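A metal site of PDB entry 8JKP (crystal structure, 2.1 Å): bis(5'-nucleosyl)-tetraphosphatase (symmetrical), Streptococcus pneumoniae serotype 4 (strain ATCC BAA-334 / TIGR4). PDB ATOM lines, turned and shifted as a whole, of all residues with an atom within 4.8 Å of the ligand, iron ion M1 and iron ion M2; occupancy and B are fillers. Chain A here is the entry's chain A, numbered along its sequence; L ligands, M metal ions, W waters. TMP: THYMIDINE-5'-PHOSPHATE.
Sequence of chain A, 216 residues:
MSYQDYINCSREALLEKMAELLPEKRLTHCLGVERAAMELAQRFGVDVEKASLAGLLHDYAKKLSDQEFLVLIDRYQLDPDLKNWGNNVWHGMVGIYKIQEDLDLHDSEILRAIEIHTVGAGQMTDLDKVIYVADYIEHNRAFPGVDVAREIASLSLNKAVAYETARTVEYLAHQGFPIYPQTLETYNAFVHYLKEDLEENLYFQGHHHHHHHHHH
OG1 of Thr 118 lies close to O2P of the ligand, 2.7 Å away.
An oxygen (O4) of the ligand is in hydrogen-bond range of the side-chain hydroxyl (OG1) of Thr 183, 2.8 Å away.
An oxygen (O2) of the ligand is in hydrogen-bond range of the side-chain amide nitrogen (ND2) of Asn 88 (3.0 Å).
The backbone NH (N) of Tyr 180 lies within hydrogen-bond range of an oxygen (O4) of the ligand, 3.2 Å away.
OG1 of Thr 118 sits close to NE2 of His 117, at 3.3 Å.
The backbone carbonyl oxygen (O) of Asn 88 is in hydrogen-bond range of a ring nitrogen (ND1) of His 91 (3.3 Å).
The side-chain carboxylate of Asp 59 sits close to the guanidinium group of Arg 26.
OG1 of Thr 183 lies close to O of Tyr 180 (3.5 Å).
The backbone carbonyl oxygen (O) of Leu 172 is in hydrogen-bond range of the backbone NH (N) of Phe 177.
Merely in contact with the ligand: Lys 62 (3.7 Å), Thr 168 (3.7 Å), Leu 172 (3.4 Å) and Phe 177 (3.9 Å).
Hydrophobic or aromatic side chains that line the ligand: His 91, His 117, Leu 172, Phe 177 and Tyr 180.
Within 4 Å of the ligand: Lys 62, Asn 88, His 91, His 117, Thr 118, Asp 135, Thr 168, Leu 172, Phe 177, Tyr 180 and Thr 183.
Merely in contact with iron ion M1: Thr 118 (3.7 Å).
The nearest printed residue that does not touch iron ion M1 is His 58 (4.02 Å).
Of the 19 residues printed, 4 come within 4 Å of iron ion M2.
The nearest printed residue that does not touch iron ion M2 is Arg 26 (4.1 Å).
Iron ion M1 is bound by NE2 of His 117 (2.0 Å), water W5 (2.0 Å), NE2 of His 91 (2.0 Å), water W6 (2.1 Å), OD1 of Asp 59 (2.1 Å) and O2P of the ligand (2.1 Å).
Iron ion M2 is bound by a ring nitrogen (NE2) of His 29 (2.0 Å), water W6 (2.0 Å), a ring nitrogen (NE2) of His 58 (2.0 Å), water W2 (2.1 Å), the side-chain carboxylate (OD1) of Asp 135 (2.1 Å) and the side-chain carboxylate (OD2) of Asp 59 (2.1 Å).
Water W5 lies within hydrogen-bond range of the side-chain amino group of Lys 62 (2.9 Å) and an oxygen (O3P) of the ligand (2.9 Å).
Water W6 lies within hydrogen-bond range of the side-chain carboxylate of Asp 135 and an oxygen (O3P) of the ligand.
Water W2 bridges an oxygen (O3P) of the ligand (2.8 Å) and the guanidinium group of Arg 26 (3.3 Å).
Water W7 bridges O1P of the ligand and OD2 of Asp 135.
Water W1 lies within hydrogen-bond range of OD2 of Asp 135, O of His 117 and O1P of the ligand.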
ATOM      1  N   ARG A  26      25.192  -9.380  19.635  1.00  0.00           N
ATOM      2  CA  ARG A  26      24.750  -9.377  18.231  1.00  0.00           C
ATOM      3  C   ARG A  26      25.022 -10.719  17.528  1.00  0.00           C
ATOM      4  O   ARG A  26      24.187 -11.210  16.761  1.00  0.00           O
ATOM      5  CB  ARG A  26      25.389  -8.204  17.458  1.00  0.00           C
ATOM      6  CG  ARG A  26      24.873  -8.037  16.010  1.00  0.00           C
ATOM      7  CD  ARG A  26      23.358  -7.836  15.912  1.00  0.00           C
ATOM      8  NE  ARG A  26      22.934  -6.679  16.694  1.00  0.00           N
ATOM      9  CZ  ARG A  26      21.713  -6.149  16.699  1.00  0.00           C
ATOM     10  NH1 ARG A  26      21.478  -5.093  17.464  1.00  0.00           N
ATOM     11  NH2 ARG A  26      20.731  -6.661  15.961  1.00  0.00           N
ATOM     12  N   HIS A  29      22.534 -13.150  18.864  1.00  0.00           N
ATOM     13  CA  HIS A  29      21.313 -12.841  18.108  1.00  0.00           C
ATOM     14  C   HIS A  29      21.315 -13.560  16.777  1.00  0.00           C
ATOM     15  O   HIS A  29      20.344 -14.236  16.462  1.00  0.00           O
ATOM     16  CB  HIS A  29      21.111 -11.322  17.925  1.00  0.00           C
ATOM     17  CG  HIS A  29      20.053 -10.951  16.922  1.00  0.00           C
ATOM     18  ND1 HIS A  29      18.717 -11.161  17.122  1.00  0.00           N
ATOM     19  CD2 HIS A  29      20.157 -10.338  15.709  1.00  0.00           C
ATOM     20  CE1 HIS A  29      18.029 -10.698  16.081  1.00  0.00           C
ATOM     21  NE2 HIS A  29      18.877 -10.181  15.199  1.00  0.00           N
ATOM     22  N   VAL A  33      18.788 -16.343  15.313  1.00  0.00           N
ATOM     23  CA  VAL A  33      18.031 -16.206  14.070  1.00  0.00           C
ATOM     24  C   VAL A  33      18.303 -17.414  13.168  1.00  0.00           C
ATOM     25  O   VAL A  33      17.384 -17.923  12.547  1.00  0.00           O
ATOM     26  CB  VAL A  33      18.271 -14.854  13.324  1.00  0.00           C
ATOM     27  CG1 VAL A  33      17.429 -14.764  12.058  1.00  0.00           C
ATOM     28  CG2 VAL A  33      17.936 -13.646  14.203  1.00  0.00           C
ATOM     29  N   HIS A  58      21.996 -12.315   8.473  1.00  0.00           N
ATOM     30  CA  HIS A  58      21.112 -11.168   8.196  1.00  0.00           C
ATOM     31  C   HIS A  58      21.636  -9.838   8.799  1.00  0.00           C
ATOM     32  O   HIS A  58      21.485  -8.790   8.181  1.00  0.00           O
ATOM     33  CB  HIS A  58      19.683 -11.429   8.659  1.00  0.00           C
ATOM     34  CG  HIS A  58      19.518 -11.260  10.130  1.00  0.00           C
ATOM     35  ND1 HIS A  58      20.103 -12.105  11.036  1.00  0.00           N
ATOM     36  CD2 HIS A  58      18.917 -10.283  10.863  1.00  0.00           C
ATOM     37  CE1 HIS A  58      19.816 -11.695  12.259  1.00  0.00           C
ATOM     38  NE2 HIS A  58      19.103 -10.570  12.198  1.00  0.00           N
ATOM     39  N   ASP A  59      22.295  -9.925   9.957  1.00  0.00           N
ATOM     40  CA  ASP A  59      22.847  -8.766  10.676  1.00  0.00           C
ATOM     41  C   ASP A  59      24.383  -8.661  10.604  1.00  0.00           C
ATOM     42  O   ASP A  59      24.993  -7.971  11.415  1.00  0.00           O
ATOM     43  CB  ASP A  59      22.385  -8.735  12.141  1.00  0.00           C
ATOM     44  CG  ASP A  59      21.050  -8.011  12.345  1.00  0.00           C
ATOM     45  OD1 ASP A  59      20.528  -7.323  11.419  1.00  0.00           O
ATOM     46  OD2 ASP A  59      20.424  -8.150  13.446  1.00  0.00           O
ATOM     47  N   LYS A  62      25.824  -5.096  10.468  1.00  0.00           N
ATOM     48  CA  LYS A  62      25.204  -4.226  11.471  1.00  0.00           C
ATOM     49  C   LYS A  62      26.153  -3.129  11.993  1.00  0.00           C
ATOM     50  O   LYS A  62      25.694  -2.025  12.278  1.00  0.00           O
ATOM     51  CB  LYS A  62      24.640  -5.051  12.636  1.00  0.00           C
ATOM     52  CG  LYS A  62      23.839  -4.292  13.690  1.00  0.00           C
ATOM     53  CD  LYS A  62      22.462  -3.832  13.212  1.00  0.00           C
ATOM     54  CE  LYS A  62      21.724  -3.152  14.351  1.00  0.00           C
ATOM     55  NZ  LYS A  62      20.256  -3.054  14.124  1.00  0.00           N
ATOM     56  N   ASN A  88      19.826   1.505  10.214  1.00  0.00           N
ATOM     57  CA  ASN A  88      18.581   0.731  10.273  1.00  0.00           C
ATOM     58  C   ASN A  88      18.165   0.242   8.880  1.00  0.00           C
ATOM     59  O   ASN A  88      17.931  -0.961   8.691  1.00  0.00           O
ATOM     60  CB  ASN A  88      17.449   1.529  10.949  1.00  0.00           C
ATOM     61  CG  ASN A  88      17.700   1.766  12.450  1.00  0.00           C
ATOM     62  OD1 ASN A  88      18.601   1.176  13.043  1.00  0.00           O
ATOM     63  ND2 ASN A  88      16.899   2.612  13.064  1.00  0.00           N
ATOM     64  N   HIS A  91      21.946  -1.608   6.850  1.00  0.00           N
ATOM     65  CA  HIS A  91      22.645  -2.869   7.208  1.00  0.00           C
ATOM     66  C   HIS A  91      22.139  -4.090   6.428  1.00  0.00           C
ATOM     67  O   HIS A  91      22.930  -4.972   6.095  1.00  0.00           O
ATOM     68  CB  HIS A  91      22.749  -3.086   8.732  1.00  0.00           C
ATOM     69  CG  HIS A  91      21.486  -3.582   9.381  1.00  0.00           C
ATOM     70  ND1 HIS A  91      20.460  -2.741   9.754  1.00  0.00           N
ATOM     71  CD2 HIS A  91      21.100  -4.825   9.773  1.00  0.00           C
ATOM     72  CE1 HIS A  91      19.499  -3.444  10.342  1.00  0.00           C
ATOM     73  NE2 HIS A  91      19.853  -4.728  10.372  1.00  0.00           N
ATOM     74  N   HIS A 117      15.238  -7.736   5.182  1.00  0.00           N
ATOM     75  CA  HIS A 117      14.950  -8.327   6.505  1.00  0.00           C
ATOM     76  C   HIS A 117      14.402  -7.300   7.512  1.00  0.00           C
ATOM     77  O   HIS A 117      13.669  -7.682   8.416  1.00  0.00           O
ATOM     78  CB  HIS A 117      16.153  -9.110   7.079  1.00  0.00           C
ATOM     79  CG  HIS A 117      17.128  -8.270   7.850  1.00  0.00           C
ATOM     80  ND1 HIS A 117      18.238  -7.722   7.270  1.00  0.00           N
ATOM     81  CD2 HIS A 117      17.154  -7.904   9.159  1.00  0.00           C
ATOM     82  CE1 HIS A 117      18.907  -7.023   8.176  1.00  0.00           C
ATOM     83  NE2 HIS A 117      18.279  -7.123   9.355  1.00  0.00           N
ATOM     84  N   THR A 118      14.730  -6.024   7.339  1.00  0.00           N
ATOM     85  CA  THR A 118      14.260  -4.953   8.245  1.00  0.00           C
ATOM     86  C   THR A 118      12.935  -4.366   7.742  1.00  0.00           C
ATOM     87  O   THR A 118      11.991  -4.237   8.509  1.00  0.00           O
ATOM     88  CB  THR A 118      15.303  -3.814   8.390  1.00  0.00           C
ATOM     89  OG1 THR A 118      16.565  -4.364   8.751  1.00  0.00           O
ATOM     90  CG2 THR A 118      14.891  -2.750   9.419  1.00  0.00           C
ATOM     91  N   VAL A 119      12.877  -4.053   6.447  1.00  0.00           N
ATOM     92  CA  VAL A 119      11.806  -3.221   5.894  1.00  0.00           C
ATOM     93  C   VAL A 119      10.733  -4.042   5.179  1.00  0.00           C
ATOM     94  O   VAL A 119       9.648  -3.535   4.920  1.00  0.00           O
ATOM     95  CB  VAL A 119      12.390  -2.090   4.970  1.00  0.00           C
ATOM     96  CG1 VAL A 119      13.296  -1.172   5.779  1.00  0.00           C
ATOM     97  CG2 VAL A 119      13.168  -2.652   3.773  1.00  0.00           C
ATOM     98  N   ASP A 135      14.003 -13.230  12.759  1.00  0.00           N
ATOM     99  CA  ASP A 135      14.666 -12.060  13.358  1.00  0.00           C
ATOM    100  C   ASP A 135      13.943 -11.571  14.628  1.00  0.00           C
ATOM    101  O   ASP A 135      14.576 -11.250  15.651  1.00  0.00           O
ATOM    102  CB  ASP A 135      14.715 -10.946  12.305  1.00  0.00           C
ATOM    103  CG  ASP A 135      15.563  -9.762  12.726  1.00  0.00           C
ATOM    104  OD1 ASP A 135      16.575  -9.893  13.495  1.00  0.00           O
ATOM    105  OD2 ASP A 135      15.252  -8.661  12.238  1.00  0.00           O
ATOM    106  N   THR A 168       6.066  -2.732  14.438  1.00  0.00           N
ATOM    107  CA  THR A 168       7.209  -1.875  14.102  1.00  0.00           C
ATOM    108  C   THR A 168       6.758  -0.483  13.677  1.00  0.00           C
ATOM    109  O   THR A 168       7.287   0.490  14.171  1.00  0.00           O
ATOM    110  CB  THR A 168       8.082  -2.553  13.042  1.00  0.00           C
ATOM    111  OG1 THR A 168       8.548  -3.780  13.595  1.00  0.00           O
ATOM    112  CG2 THR A 168       9.297  -1.709  12.626  1.00  0.00           C
ATOM    113  N   LEU A 172       7.667   2.861  15.730  1.00  0.00           N
ATOM    114  CA  LEU A 172       8.385   3.988  15.110  1.00  0.00           C
ATOM    115  C   LEU A 172       7.607   5.306  15.206  1.00  0.00           C
ATOM    116  O   LEU A 172       8.184   6.354  15.524  1.00  0.00           O
ATOM    117  CB  LEU A 172       8.793   3.677  13.657  1.00  0.00           C
ATOM    118  CG  LEU A 172       9.807   2.531  13.477  1.00  0.00           C
ATOM    119  CD1 LEU A 172       9.933   2.134  12.008  1.00  0.00           C
ATOM    120  CD2 LEU A 172      11.171   2.888  14.063  1.00  0.00           C
ATOM    121  N   PHE A 177      10.002   8.430  15.045  1.00  0.00           N
ATOM    122  CA  PHE A 177      11.115   8.084  14.170  1.00  0.00           C
ATOM    123  C   PHE A 177      10.693   7.992  12.706  1.00  0.00           C
ATOM    124  O   PHE A 177       9.604   7.503  12.424  1.00  0.00           O
ATOM    125  CB  PHE A 177      11.729   6.768  14.638  1.00  0.00           C
ATOM    126  CG  PHE A 177      13.199   6.731  14.483  1.00  0.00           C
ATOM    127  CD1 PHE A 177      14.024   7.447  15.360  1.00  0.00           C
ATOM    128  CD2 PHE A 177      13.776   6.037  13.423  1.00  0.00           C
ATOM    129  CE1 PHE A 177      15.407   7.437  15.201  1.00  0.00           C
ATOM    130  CE2 PHE A 177      15.166   6.015  13.254  1.00  0.00           C
ATOM    131  CZ  PHE A 177      15.983   6.719  14.149  1.00  0.00           C
ATOM    132  N   PRO A 178      11.554   8.449  11.766  1.00  0.00           N
ATOM    133  CA  PRO A 178      11.185   8.290  10.345  1.00  0.00           C
ATOM    134  C   PRO A 178      10.941   6.827   9.995  1.00  0.00           C
ATOM    135  O   PRO A 178      11.543   5.931  10.600  1.00  0.00           O
ATOM    136  CB  PRO A 178      12.406   8.831   9.580  1.00  0.00           C
ATOM    137  CG  PRO A 178      13.158   9.663  10.573  1.00  0.00           C
ATOM    138  CD  PRO A 178      12.880   9.074  11.919  1.00  0.00           C
ATOM    139  N   ILE A 179      10.020   6.608   9.073  1.00  0.00           N
ATOM    140  CA  ILE A 179       9.653   5.261   8.643  1.00  0.00           C
ATOM    141  C   ILE A 179       9.955   5.100   7.169  1.00  0.00           C
ATOM    142  O   ILE A 179       9.386   5.803   6.319  1.00  0.00           O
ATOM    143  CB  ILE A 179       8.148   4.961   8.880  1.00  0.00           C
ATOM    144  CG1 ILE A 179       7.809   4.955  10.375  1.00  0.00           C
ATOM    145  CG2 ILE A 179       7.730   3.647   8.197  1.00  0.00           C
ATOM    146  CD1 ILE A 179       6.352   5.231  10.679  1.00  0.00           C
ATOM    147  N   TYR A 180      10.835   4.153   6.856  1.00  0.00           N
ATOM    148  CA  TYR A 180      11.221   3.936   5.473  1.00  0.00           C
ATOM    149  C   TYR A 180       9.989   3.570   4.624  1.00  0.00           C
ATOM    150  O   TYR A 180       9.204   2.747   5.056  1.00  0.00           O
ATOM    151  CB  TYR A 180      12.282   2.848   5.392  1.00  0.00           C
ATOM    152  CG  TYR A 180      12.947   2.789   4.056  1.00  0.00           C
ATOM    153  CD1 TYR A 180      13.764   3.845   3.610  1.00  0.00           C
ATOM    154  CD2 TYR A 180      12.768   1.683   3.222  1.00  0.00           C
ATOM    155  CE1 TYR A 180      14.378   3.798   2.368  1.00  0.00           C
ATOM    156  CE2 TYR A 180      13.399   1.628   1.983  1.00  0.00           C
ATOM    157  CZ  TYR A 180      14.184   2.693   1.563  1.00  0.00           C
ATOM    158  OH  TYR A 180      14.793   2.643   0.340  1.00  0.00           O
ATOM    159  N   THR A 183       8.787  -0.084   4.085  1.00  0.00           N
ATOM    160  CA  THR A 183       8.129  -0.651   5.277  1.00  0.00           C
ATOM    161  C   THR A 183       6.598  -0.525   5.196  1.00  0.00           C
ATOM    162  O   THR A 183       5.862  -1.461   5.540  1.00  0.00           O
ATOM    163  CB  THR A 183       8.636   0.008   6.577  1.00  0.00           C
ATOM    164  OG1 THR A 183      10.047  -0.204   6.674  1.00  0.00           O
ATOM    165  CG2 THR A 183       7.930  -0.545   7.843  1.00  0.00           C
HETATM  166  P   TMP L   1      16.031  -4.966  12.513  1.00  0.00           P
HETATM  167  O1P TMP L   1      14.623  -5.455  12.208  1.00  0.00           O
HETATM  168  O2P TMP L   1      17.003  -5.083  11.332  1.00  0.00           O
HETATM  169  O3P TMP L   1      16.583  -5.528  13.811  1.00  0.00           O
HETATM  170  O5' TMP L   1      15.775  -3.394  12.747  1.00  0.00           O
HETATM  171  C5' TMP L   1      16.673  -2.564  13.469  1.00  0.00           C
HETATM  172  C4' TMP L   1      16.011  -1.221  13.777  1.00  0.00           C
HETATM  173  O4' TMP L   1      15.570  -0.585  12.573  1.00  0.00           O
HETATM  174  C3' TMP L   1      14.814  -1.328  14.698  1.00  0.00           C
HETATM  175  O3' TMP L   1      15.155  -0.715  15.928  1.00  0.00           O
HETATM  176  C2' TMP L   1      13.703  -0.513  14.053  1.00  0.00           C
HETATM  177  C1' TMP L   1      14.401   0.168  12.875  1.00  0.00           C
HETATM  178  N1  TMP L   1      13.543   0.369  11.693  1.00  0.00           N
HETATM  179  C2  TMP L   1      13.556   1.667  11.131  1.00  0.00           C
HETATM  180  O2  TMP L   1      14.284   2.542  11.631  1.00  0.00           O
HETATM  181  N3  TMP L   1      12.828   2.017  10.078  1.00  0.00           N
HETATM  182  C4  TMP L   1      12.053   1.113   9.503  1.00  0.00           C
HETATM  183  O4  TMP L   1      11.399   1.479   8.528  1.00  0.00           O
HETATM  184  C5  TMP L   1      11.997  -0.278  10.064  1.00  0.00           C
HETATM  185  C5M TMP L   1      11.133  -1.353   9.480  1.00  0.00           C
HETATM  186  C6  TMP L   1      12.766  -0.593  11.182  1.00  0.00           C
HETATM  187 FE    FE M   1      18.749  -6.269  11.106  1.00  0.00          FE
HETATM  188 FE    FE M   2      18.536  -9.130  13.535  1.00  0.00          FE
HETATM  189  O   HOH W   1      13.098  -7.827  10.988  1.00  0.00           O
HETATM  190  O   HOH W   2      17.813  -7.814  14.938  1.00  0.00           O
HETATM  191  O   HOH W   3      15.970  -4.864  16.186  1.00  0.00           O
HETATM  192  O   HOH W   4      12.605  -3.718  12.393  1.00  0.00           O
HETATM  193  O   HOH W   5      19.378  -5.500  12.878  1.00  0.00           O
HETATM  194  O   HOH W   6      17.852  -7.759  12.207  1.00  0.00           O
HETATM  195  O   HOH W   7      13.458  -7.060  14.403  1.00  0.00           O
